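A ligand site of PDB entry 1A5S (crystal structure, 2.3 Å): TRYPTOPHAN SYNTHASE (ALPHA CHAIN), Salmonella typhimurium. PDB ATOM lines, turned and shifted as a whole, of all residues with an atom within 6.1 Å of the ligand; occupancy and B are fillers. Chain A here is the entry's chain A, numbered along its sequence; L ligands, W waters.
Water W1 lies within hydrogen-bond range of N of Ala 236 (2.5 Å), O2 of the ligand (2.6 Å), O of Ile 214 (3.1 Å) and N of Ser 235 (3.2 Å).
Merely in contact with the ligand: Ile 153 (2.9 Å), Phe 212 (3.0 Å), Tyr 175 (3.1 Å), Thr 183 (3.3 Å), Phe 22 (3.6 Å), Leu 100 (3.7 Å), Ala 59 (3.8 Å), Ile 232 (3.9 Å), Ser 233 (3.9 Å) and Ala 129 (3.9 Å).
Hydrophobic or aromatic side chains that line the ligand: Phe 22, Ala 59, Leu 100, Ala 129, Ile 153, Tyr 175, Phe 212 and Ile 232.
15 residues have an atom within 4 Å of the ligand: Phe 22, Ala 59, Asp 60, Leu 100, Ala 129, Ile 153, Tyr 175, Thr 183, Gly 184, Phe 212, Gly 213, Ile 232, Ser 233, Gly 234 and Ser 235.
O1 of the ligand sits at hydrogen-bond distance from N of Ser 235, at 2.8 Å.
O1 of the ligand is in hydrogen-bond range of OG of Ser 235 (2.6 Å).
The side-chain carboxylate (OD1) of Asp 60 is in hydrogen-bond range of a nitrogen (N1) of the ligand, 2.7 Å away.
N of Gly 213 is in hydrogen-bond range of O3 of the ligand (2.7 Å).
O2 of the ligand is in hydrogen-bond range of N of Gly 234 (2.9 Å).
N of Gly 184 lies within hydrogen-bond range of O3 of the ligand (3.3 Å).
The side-chain carboxylate (OD1) of Asp 60 sits at hydrogen-bond distance from the side-chain hydroxyl (OG1) of Thr 183, 3.1 Å away.
The side-chain hydroxyl (OH) of Tyr 102 sits at hydrogen-bond distance from the side-chain carboxylate (OD2) of Asp 60 (2.6 Å).
O of Gly 184 is in hydrogen-bond range of NH2 of Arg 179, at 3.0 Å.
N of Thr 183 lies within hydrogen-bond range of O of Ala 59 (3.2 Å).
The backbone carbonyl oxygen (O) of Ser 233 is in hydrogen-bond range of the backbone NH (N) of Phe 22, at 2.9 Å.
The side-chain hydroxyl (OH) of Tyr 102 is in hydrogen-bond range of the backbone NH (N) of Ala 59 (3.0 Å).
O of Ile 214 sits at hydrogen-bond distance from OG of Ser 233, 3.1 Å away.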
ATOM      1  N   PHE A  22     -16.965  11.092 -20.417  1.00  0.00           N
ATOM      2  CA  PHE A  22     -17.331  12.298 -19.689  1.00  0.00           C
ATOM      3  C   PHE A  22     -16.160  13.252 -19.823  1.00  0.00           C
ATOM      4  O   PHE A  22     -15.009  12.837 -19.824  1.00  0.00           O
ATOM      5  CB  PHE A  22     -17.567  12.041 -18.210  1.00  0.00           C
ATOM      6  CG  PHE A  22     -17.501  13.300 -17.365  1.00  0.00           C
ATOM      7  CD1 PHE A  22     -16.289  13.962 -17.190  1.00  0.00           C
ATOM      8  CD2 PHE A  22     -18.647  13.849 -16.824  1.00  0.00           C
ATOM      9  CE1 PHE A  22     -16.231  15.149 -16.490  1.00  0.00           C
ATOM     10  CE2 PHE A  22     -18.586  15.043 -16.119  1.00  0.00           C
ATOM     11  CZ  PHE A  22     -17.380  15.690 -15.955  1.00  0.00           C
ATOM     12  N   GLU A  49     -21.542  12.591 -21.396  1.00  0.00           N
ATOM     13  CA  GLU A  49     -21.751  13.007 -20.014  1.00  0.00           C
ATOM     14  C   GLU A  49     -20.907  14.274 -19.914  1.00  0.00           C
ATOM     15  O   GLU A  49     -19.681  14.237 -20.018  1.00  0.00           O
ATOM     16  CB  GLU A  49     -21.283  11.933 -19.027  1.00  0.00           C
ATOM     17  CG  GLU A  49     -21.868  12.081 -17.633  1.00  0.00           C
ATOM     18  CD  GLU A  49     -23.387  12.023 -17.619  1.00  0.00           C
ATOM     19  OE1 GLU A  49     -23.976  11.244 -18.388  1.00  0.00           O
ATOM     20  OE2 GLU A  49     -24.000  12.766 -16.820  1.00  0.00           O
ATOM     21  N   ALA A  59     -17.194  16.020  -5.308  1.00  0.00           N
ATOM     22  CA  ALA A  59     -17.298  14.610  -5.668  1.00  0.00           C
ATOM     23  C   ALA A  59     -16.231  14.208  -6.674  1.00  0.00           C
ATOM     24  O   ALA A  59     -16.187  13.060  -7.115  1.00  0.00           O
ATOM     25  CB  ALA A  59     -18.678  14.312  -6.227  1.00  0.00           C
ATOM     26  N   ASP A  60     -15.364  15.147  -7.033  1.00  0.00           N
ATOM     27  CA  ASP A  60     -14.336  14.904  -8.032  1.00  0.00           C
ATOM     28  C   ASP A  60     -12.904  14.816  -7.522  1.00  0.00           C
ATOM     29  O   ASP A  60     -12.495  15.541  -6.628  1.00  0.00           O
ATOM     30  CB  ASP A  60     -14.403  15.982  -9.101  1.00  0.00           C
ATOM     31  CG  ASP A  60     -15.629  15.866  -9.972  1.00  0.00           C
ATOM     32  OD1 ASP A  60     -15.791  14.816 -10.633  1.00  0.00           O
ATOM     33  OD2 ASP A  60     -16.439  16.820  -9.986  1.00  0.00           O
ATOM     34  N   ILE A  64     -10.343  15.657 -12.604  1.00  0.00           N
ATOM     35  CA  ILE A  64     -11.491  16.496 -12.938  1.00  0.00           C
ATOM     36  C   ILE A  64     -11.355  17.883 -12.319  1.00  0.00           C
ATOM     37  O   ILE A  64     -11.668  18.887 -12.954  1.00  0.00           O
ATOM     38  CB  ILE A  64     -12.821  15.877 -12.451  1.00  0.00           C
ATOM     39  CG1 ILE A  64     -12.957  14.448 -12.959  1.00  0.00           C
ATOM     40  CG2 ILE A  64     -14.009  16.711 -12.947  1.00  0.00           C
ATOM     41  CD1 ILE A  64     -13.312  14.351 -14.416  1.00  0.00           C
ATOM     42  N   LEU A 100     -23.656  16.535 -15.746  1.00  0.00           N
ATOM     43  CA  LEU A 100     -23.156  16.206 -14.408  1.00  0.00           C
ATOM     44  C   LEU A 100     -23.119  17.568 -13.734  1.00  0.00           C
ATOM     45  O   LEU A 100     -22.273  18.394 -14.055  1.00  0.00           O
ATOM     46  CB  LEU A 100     -21.747  15.610 -14.478  1.00  0.00           C
ATOM     47  CG  LEU A 100     -21.253  14.920 -13.204  1.00  0.00           C
ATOM     48  CD1 LEU A 100     -20.968  15.942 -12.121  1.00  0.00           C
ATOM     49  CD2 LEU A 100     -22.307  13.932 -12.725  1.00  0.00           C
ATOM     50  N   TYR A 102     -23.634  20.221 -10.071  1.00  0.00           N
ATOM     51  CA  TYR A 102     -23.514  20.355  -8.632  1.00  0.00           C
ATOM     52  C   TYR A 102     -24.727  21.193  -8.258  1.00  0.00           C
ATOM     53  O   TYR A 102     -25.054  22.176  -8.927  1.00  0.00           O
ATOM     54  CB  TYR A 102     -22.177  21.016  -8.247  1.00  0.00           C
ATOM     55  CG  TYR A 102     -21.067  19.991  -8.154  1.00  0.00           C
ATOM     56  CD1 TYR A 102     -20.971  19.145  -7.059  1.00  0.00           C
ATOM     57  CD2 TYR A 102     -20.165  19.815  -9.187  1.00  0.00           C
ATOM     58  CE1 TYR A 102     -20.019  18.150  -7.001  1.00  0.00           C
ATOM     59  CE2 TYR A 102     -19.203  18.817  -9.149  1.00  0.00           C
ATOM     60  CZ  TYR A 102     -19.140  17.984  -8.051  1.00  0.00           C
ATOM     61  OH  TYR A 102     -18.209  16.965  -8.020  1.00  0.00           O
ATOM     62  N   LEU A 127     -27.731  14.701 -13.685  1.00  0.00           N
ATOM     63  CA  LEU A 127     -27.345  13.997 -12.471  1.00  0.00           C
ATOM     64  C   LEU A 127     -26.738  15.075 -11.579  1.00  0.00           C
ATOM     65  O   LEU A 127     -25.774  15.735 -11.978  1.00  0.00           O
ATOM     66  CB  LEU A 127     -26.292  12.910 -12.773  1.00  0.00           C
ATOM     67  CG  LEU A 127     -25.432  12.310 -11.639  1.00  0.00           C
ATOM     68  CD1 LEU A 127     -26.317  11.733 -10.553  1.00  0.00           C
ATOM     69  CD2 LEU A 127     -24.548  11.219 -12.206  1.00  0.00           C
ATOM     70  N   ALA A 129     -24.657  15.662  -8.596  1.00  0.00           N
ATOM     71  CA  ALA A 129     -23.727  14.977  -7.708  1.00  0.00           C
ATOM     72  C   ALA A 129     -24.042  15.036  -6.214  1.00  0.00           C
ATOM     73  O   ALA A 129     -24.091  14.001  -5.555  1.00  0.00           O
ATOM     74  CB  ALA A 129     -22.321  15.494  -7.981  1.00  0.00           C
ATOM     75  N   ILE A 153     -27.768   8.058  -8.382  1.00  0.00           N
ATOM     76  CA  ILE A 153     -26.602   7.228  -8.141  1.00  0.00           C
ATOM     77  C   ILE A 153     -26.911   6.057  -7.221  1.00  0.00           C
ATOM     78  O   ILE A 153     -27.556   6.211  -6.187  1.00  0.00           O
ATOM     79  CB  ILE A 153     -25.464   8.045  -7.531  1.00  0.00           C
ATOM     80  CG1 ILE A 153     -25.145   9.239  -8.434  1.00  0.00           C
ATOM     81  CG2 ILE A 153     -24.247   7.172  -7.316  1.00  0.00           C
ATOM     82  CD1 ILE A 153     -23.725   9.770  -8.313  1.00  0.00           C
ATOM     83  N   TYR A 175     -27.103   5.444 -12.467  1.00  0.00           N
ATOM     84  CA  TYR A 175     -25.661   5.551 -12.325  1.00  0.00           C
ATOM     85  C   TYR A 175     -25.163   4.600 -11.253  1.00  0.00           C
ATOM     86  O   TYR A 175     -25.423   4.798 -10.064  1.00  0.00           O
ATOM     87  CB  TYR A 175     -25.249   6.985 -11.983  1.00  0.00           C
ATOM     88  CG  TYR A 175     -23.759   7.207 -12.022  1.00  0.00           C
ATOM     89  CD1 TYR A 175     -22.955   6.872 -10.941  1.00  0.00           C
ATOM     90  CD2 TYR A 175     -23.154   7.732 -13.156  1.00  0.00           C
ATOM     91  CE1 TYR A 175     -21.579   7.052 -10.999  1.00  0.00           C
ATOM     92  CE2 TYR A 175     -21.778   7.913 -13.214  1.00  0.00           C
ATOM     93  CZ  TYR A 175     -20.997   7.570 -12.128  1.00  0.00           C
ATOM     94  OH  TYR A 175     -19.640   7.740 -12.195  1.00  0.00           O
ATOM     95  N   LEU A 177     -22.346   3.249  -9.092  1.00  0.00           N
ATOM     96  CA  LEU A 177     -21.047   3.615  -8.540  1.00  0.00           C
ATOM     97  C   LEU A 177     -20.180   2.374  -8.409  1.00  0.00           C
ATOM     98  O   LEU A 177     -20.489   1.470  -7.631  1.00  0.00           O
ATOM     99  CB  LEU A 177     -21.244   4.255  -7.164  1.00  0.00           C
ATOM    100  CG  LEU A 177     -20.330   5.429  -6.825  1.00  0.00           C
ATOM    101  CD1 LEU A 177     -20.046   6.260  -8.070  1.00  0.00           C
ATOM    102  CD2 LEU A 177     -20.996   6.265  -5.747  1.00  0.00           C
ATOM    103  N   ARG A 179     -17.443   2.111  -7.006  1.00  0.00           N
ATOM    104  CA  ARG A 179     -16.852   2.070  -5.663  1.00  0.00           C
ATOM    105  C   ARG A 179     -17.135   3.369  -4.912  1.00  0.00           C
ATOM    106  O   ARG A 179     -17.873   4.223  -5.399  1.00  0.00           O
ATOM    107  CB  ARG A 179     -15.337   1.890  -5.781  1.00  0.00           C
ATOM    108  CG  ARG A 179     -14.720   2.736  -6.873  1.00  0.00           C
ATOM    109  CD  ARG A 179     -13.461   3.400  -6.377  1.00  0.00           C
ATOM    110  NE  ARG A 179     -12.812   4.216  -7.395  1.00  0.00           N
ATOM    111  CZ  ARG A 179     -12.892   5.546  -7.437  1.00  0.00           C
ATOM    112  NH1 ARG A 179     -13.584   6.196  -6.520  1.00  0.00           N
ATOM    113  NH2 ARG A 179     -12.249   6.220  -8.386  1.00  0.00           N
ATOM    114  N   VAL A 182     -14.027   9.284  -4.686  1.00  0.00           N
ATOM    115  CA  VAL A 182     -14.417  10.248  -5.698  1.00  0.00           C
ATOM    116  C   VAL A 182     -13.934   9.845  -7.080  1.00  0.00           C
ATOM    117  O   VAL A 182     -13.323   8.789  -7.253  1.00  0.00           O
ATOM    118  CB  VAL A 182     -13.880  11.662  -5.349  1.00  0.00           C
ATOM    119  CG1 VAL A 182     -14.384  12.093  -3.990  1.00  0.00           C
ATOM    120  CG2 VAL A 182     -12.368  11.671  -5.401  1.00  0.00           C
ATOM    121  N   THR A 183     -14.216  10.696  -8.075  1.00  0.00           N
ATOM    122  CA  THR A 183     -13.805  10.404  -9.440  1.00  0.00           C
ATOM    123  C   THR A 183     -12.271  10.328  -9.532  1.00  0.00           C
ATOM    124  O   THR A 183     -11.565  11.239  -9.111  1.00  0.00           O
ATOM    125  CB  THR A 183     -14.296  11.479 -10.434  1.00  0.00           C
ATOM    126  OG1 THR A 183     -13.609  12.710 -10.195  1.00  0.00           O
ATOM    127  CG2 THR A 183     -15.798  11.690 -10.293  1.00  0.00           C
ATOM    128  N   GLY A 184     -11.777   9.221 -10.080  1.00  0.00           N
ATOM    129  CA  GLY A 184     -10.353   9.035 -10.226  1.00  0.00           C
ATOM    130  C   GLY A 184     -10.038   7.797 -11.040  1.00  0.00           C
ATOM    131  O   GLY A 184     -10.374   6.688 -10.625  1.00  0.00           O
ATOM    132  N   ALA A 185      -9.421   7.989 -12.199  1.00  0.00           N
ATOM    133  CA  ALA A 185      -9.057   6.891 -13.085  1.00  0.00           C
ATOM    134  C   ALA A 185      -8.050   5.964 -12.395  1.00  0.00           C
ATOM    135  O   ALA A 185      -7.836   4.821 -12.820  1.00  0.00           O
ATOM    136  CB  ALA A 185      -8.465   7.424 -14.382  1.00  0.00           C
ATOM    137  N   GLY A 211     -19.827   3.584 -13.376  1.00  0.00           N
ATOM    138  CA  GLY A 211     -18.852   4.652 -13.423  1.00  0.00           C
ATOM    139  C   GLY A 211     -17.916   4.720 -12.232  1.00  0.00           C
ATOM    140  O   GLY A 211     -18.178   4.139 -11.171  1.00  0.00           O
ATOM    141  N   PHE A 212     -16.805   5.436 -12.422  1.00  0.00           N
ATOM    142  CA  PHE A 212     -15.761   5.620 -11.412  1.00  0.00           C
ATOM    143  C   PHE A 212     -14.643   4.599 -11.576  1.00  0.00           C
ATOM    144  O   PHE A 212     -14.831   3.413 -11.305  1.00  0.00           O
ATOM    145  CB  PHE A 212     -16.331   5.540  -9.990  1.00  0.00           C
ATOM    146  CG  PHE A 212     -16.651   6.874  -9.370  1.00  0.00           C
ATOM    147  CD1 PHE A 212     -16.919   7.991 -10.162  1.00  0.00           C
ATOM    148  CD2 PHE A 212     -16.689   7.025  -7.984  1.00  0.00           C
ATOM    149  CE1 PHE A 212     -17.232   9.222  -9.585  1.00  0.00           C
ATOM    150  CE2 PHE A 212     -16.992   8.267  -7.409  1.00  0.00           C
ATOM    151  CZ  PHE A 212     -17.263   9.354  -8.214  1.00  0.00           C
ATOM    152  N   GLY A 213     -13.483   5.048 -12.055  1.00  0.00           N
ATOM    153  CA  GLY A 213     -12.361   4.152 -12.212  1.00  0.00           C
ATOM    154  C   GLY A 213     -12.286   3.336 -13.496  1.00  0.00           C
ATOM    155  O   GLY A 213     -11.356   2.554 -13.674  1.00  0.00           O
ATOM    156  N   ILE A 214     -13.263   3.492 -14.379  1.00  0.00           N
ATOM    157  CA  ILE A 214     -13.246   2.746 -15.634  1.00  0.00           C
ATOM    158  C   ILE A 214     -12.266   3.364 -16.619  1.00  0.00           C
ATOM    159  O   ILE A 214     -12.468   4.494 -17.081  1.00  0.00           O
ATOM    160  CB  ILE A 214     -14.636   2.731 -16.297  1.00  0.00           C
ATOM    161  CG1 ILE A 214     -15.706   2.343 -15.283  1.00  0.00           C
ATOM    162  CG2 ILE A 214     -14.624   1.782 -17.475  1.00  0.00           C
ATOM    163  CD1 ILE A 214     -15.837   0.855 -15.068  1.00  0.00           C
ATOM    164  N   ILE A 232     -19.402   4.475 -17.999  1.00  0.00           N
ATOM    165  CA  ILE A 232     -19.015   5.873 -18.140  1.00  0.00           C
ATOM    166  C   ILE A 232     -17.541   5.969 -17.722  1.00  0.00           C
ATOM    167  O   ILE A 232     -17.114   5.350 -16.748  1.00  0.00           O
ATOM    168  CB  ILE A 232     -19.855   6.785 -17.221  1.00  0.00           C
ATOM    169  CG1 ILE A 232     -21.285   6.898 -17.747  1.00  0.00           C
ATOM    170  CG2 ILE A 232     -19.227   8.160 -17.137  1.00  0.00           C
ATOM    171  CD1 ILE A 232     -22.334   6.926 -16.663  1.00  0.00           C
ATOM    172  N   SER A 233     -16.762   6.737 -18.487  1.00  0.00           N
ATOM    173  CA  SER A 233     -15.346   6.908 -18.205  1.00  0.00           C
ATOM    174  C   SER A 233     -15.000   8.385 -18.355  1.00  0.00           C
ATOM    175  O   SER A 233     -15.199   8.965 -19.428  1.00  0.00           O
ATOM    176  CB  SER A 233     -14.508   6.069 -19.184  1.00  0.00           C
ATOM    177  OG  SER A 233     -13.199   6.581 -19.324  1.00  0.00           O
ATOM    178  N   GLY A 234     -14.499   8.995 -17.293  1.00  0.00           N
ATOM    179  CA  GLY A 234     -14.160  10.405 -17.333  1.00  0.00           C
ATOM    180  C   GLY A 234     -12.698  10.759 -17.126  1.00  0.00           C
ATOM    181  O   GLY A 234     -12.049  11.296 -18.021  1.00  0.00           O
ATOM    182  N   SER A 235     -12.169  10.458 -15.947  1.00  0.00           N
ATOM    183  CA  SER A 235     -10.765  10.772 -15.653  1.00  0.00           C
ATOM    184  C   SER A 235      -9.827  10.228 -16.730  1.00  0.00           C
ATOM    185  O   SER A 235      -8.880  10.914 -17.134  1.00  0.00           O
ATOM    186  CB  SER A 235     -10.384  10.217 -14.281  1.00  0.00           C
ATOM    187  OG  SER A 235     -11.036  10.943 -13.244  1.00  0.00           O
ATOM    188  N   ALA A 236     -10.082   9.003 -17.175  1.00  0.00           N
ATOM    189  CA  ALA A 236      -9.259   8.387 -18.213  1.00  0.00           C
ATOM    190  C   ALA A 236      -9.202   9.282 -19.446  1.00  0.00           C
ATOM    191  O   ALA A 236      -8.134   9.510 -20.002  1.00  0.00           O
ATOM    192  CB  ALA A 236      -9.823   7.007 -18.589  1.00  0.00           C
HETATM  193  C1  LIG L   1     -18.366  11.959 -13.243  1.00  0.00           C
HETATM  194  C2  LIG L   1     -19.008  12.017 -11.962  1.00  0.00           C
HETATM  195  C3  LIG L   1     -18.579  13.208 -11.343  1.00  0.00           C
HETATM  196  C4  LIG L   1     -19.907  11.186 -11.287  1.00  0.00           C
HETATM  197  C5  LIG L   1     -17.586  13.071 -13.340  1.00  0.00           C
HETATM  198  N1  LIG L   1     -17.723  13.837 -12.200  1.00  0.00           N
HETATM  199  C6  LIG L   1     -19.020  13.585 -10.073  1.00  0.00           C
HETATM  200  C7  LIG L   1     -20.352  11.564 -10.034  1.00  0.00           C
HETATM  201  C8  LIG L   1     -19.907  12.755  -9.442  1.00  0.00           C
HETATM  202  F1  LIG L   1     -21.220  10.796  -9.391  1.00  0.00           F
HETATM  203  C9  LIG L   1     -18.502  10.880 -14.268  1.00  0.00           C
HETATM  204  C10 LIG L   1     -17.752   9.639 -13.839  1.00  0.00           C
HETATM  205  C11 LIG L   1     -16.242   9.885 -13.851  1.00  0.00           C
HETATM  206  P1  LIG L   1     -13.954   8.575 -13.437  1.00  0.00           P
HETATM  207  O1  LIG L   1     -13.401   9.949 -13.449  1.00  0.00           O
HETATM  208  O2  LIG L   1     -13.681   7.845 -14.705  1.00  0.00           O
HETATM  209  O3  LIG L   1     -13.818   7.764 -12.181  1.00  0.00           O
HETATM  210  O4  LIG L   1     -15.580   8.722 -13.403  1.00  0.00           O
HETATM  211  O   HOH W   1     -11.601   7.336 -16.159  1.00  0.00           O
HETATM  212  O   HOH W   2     -15.300   5.479 -14.798  1.00  0.00           O
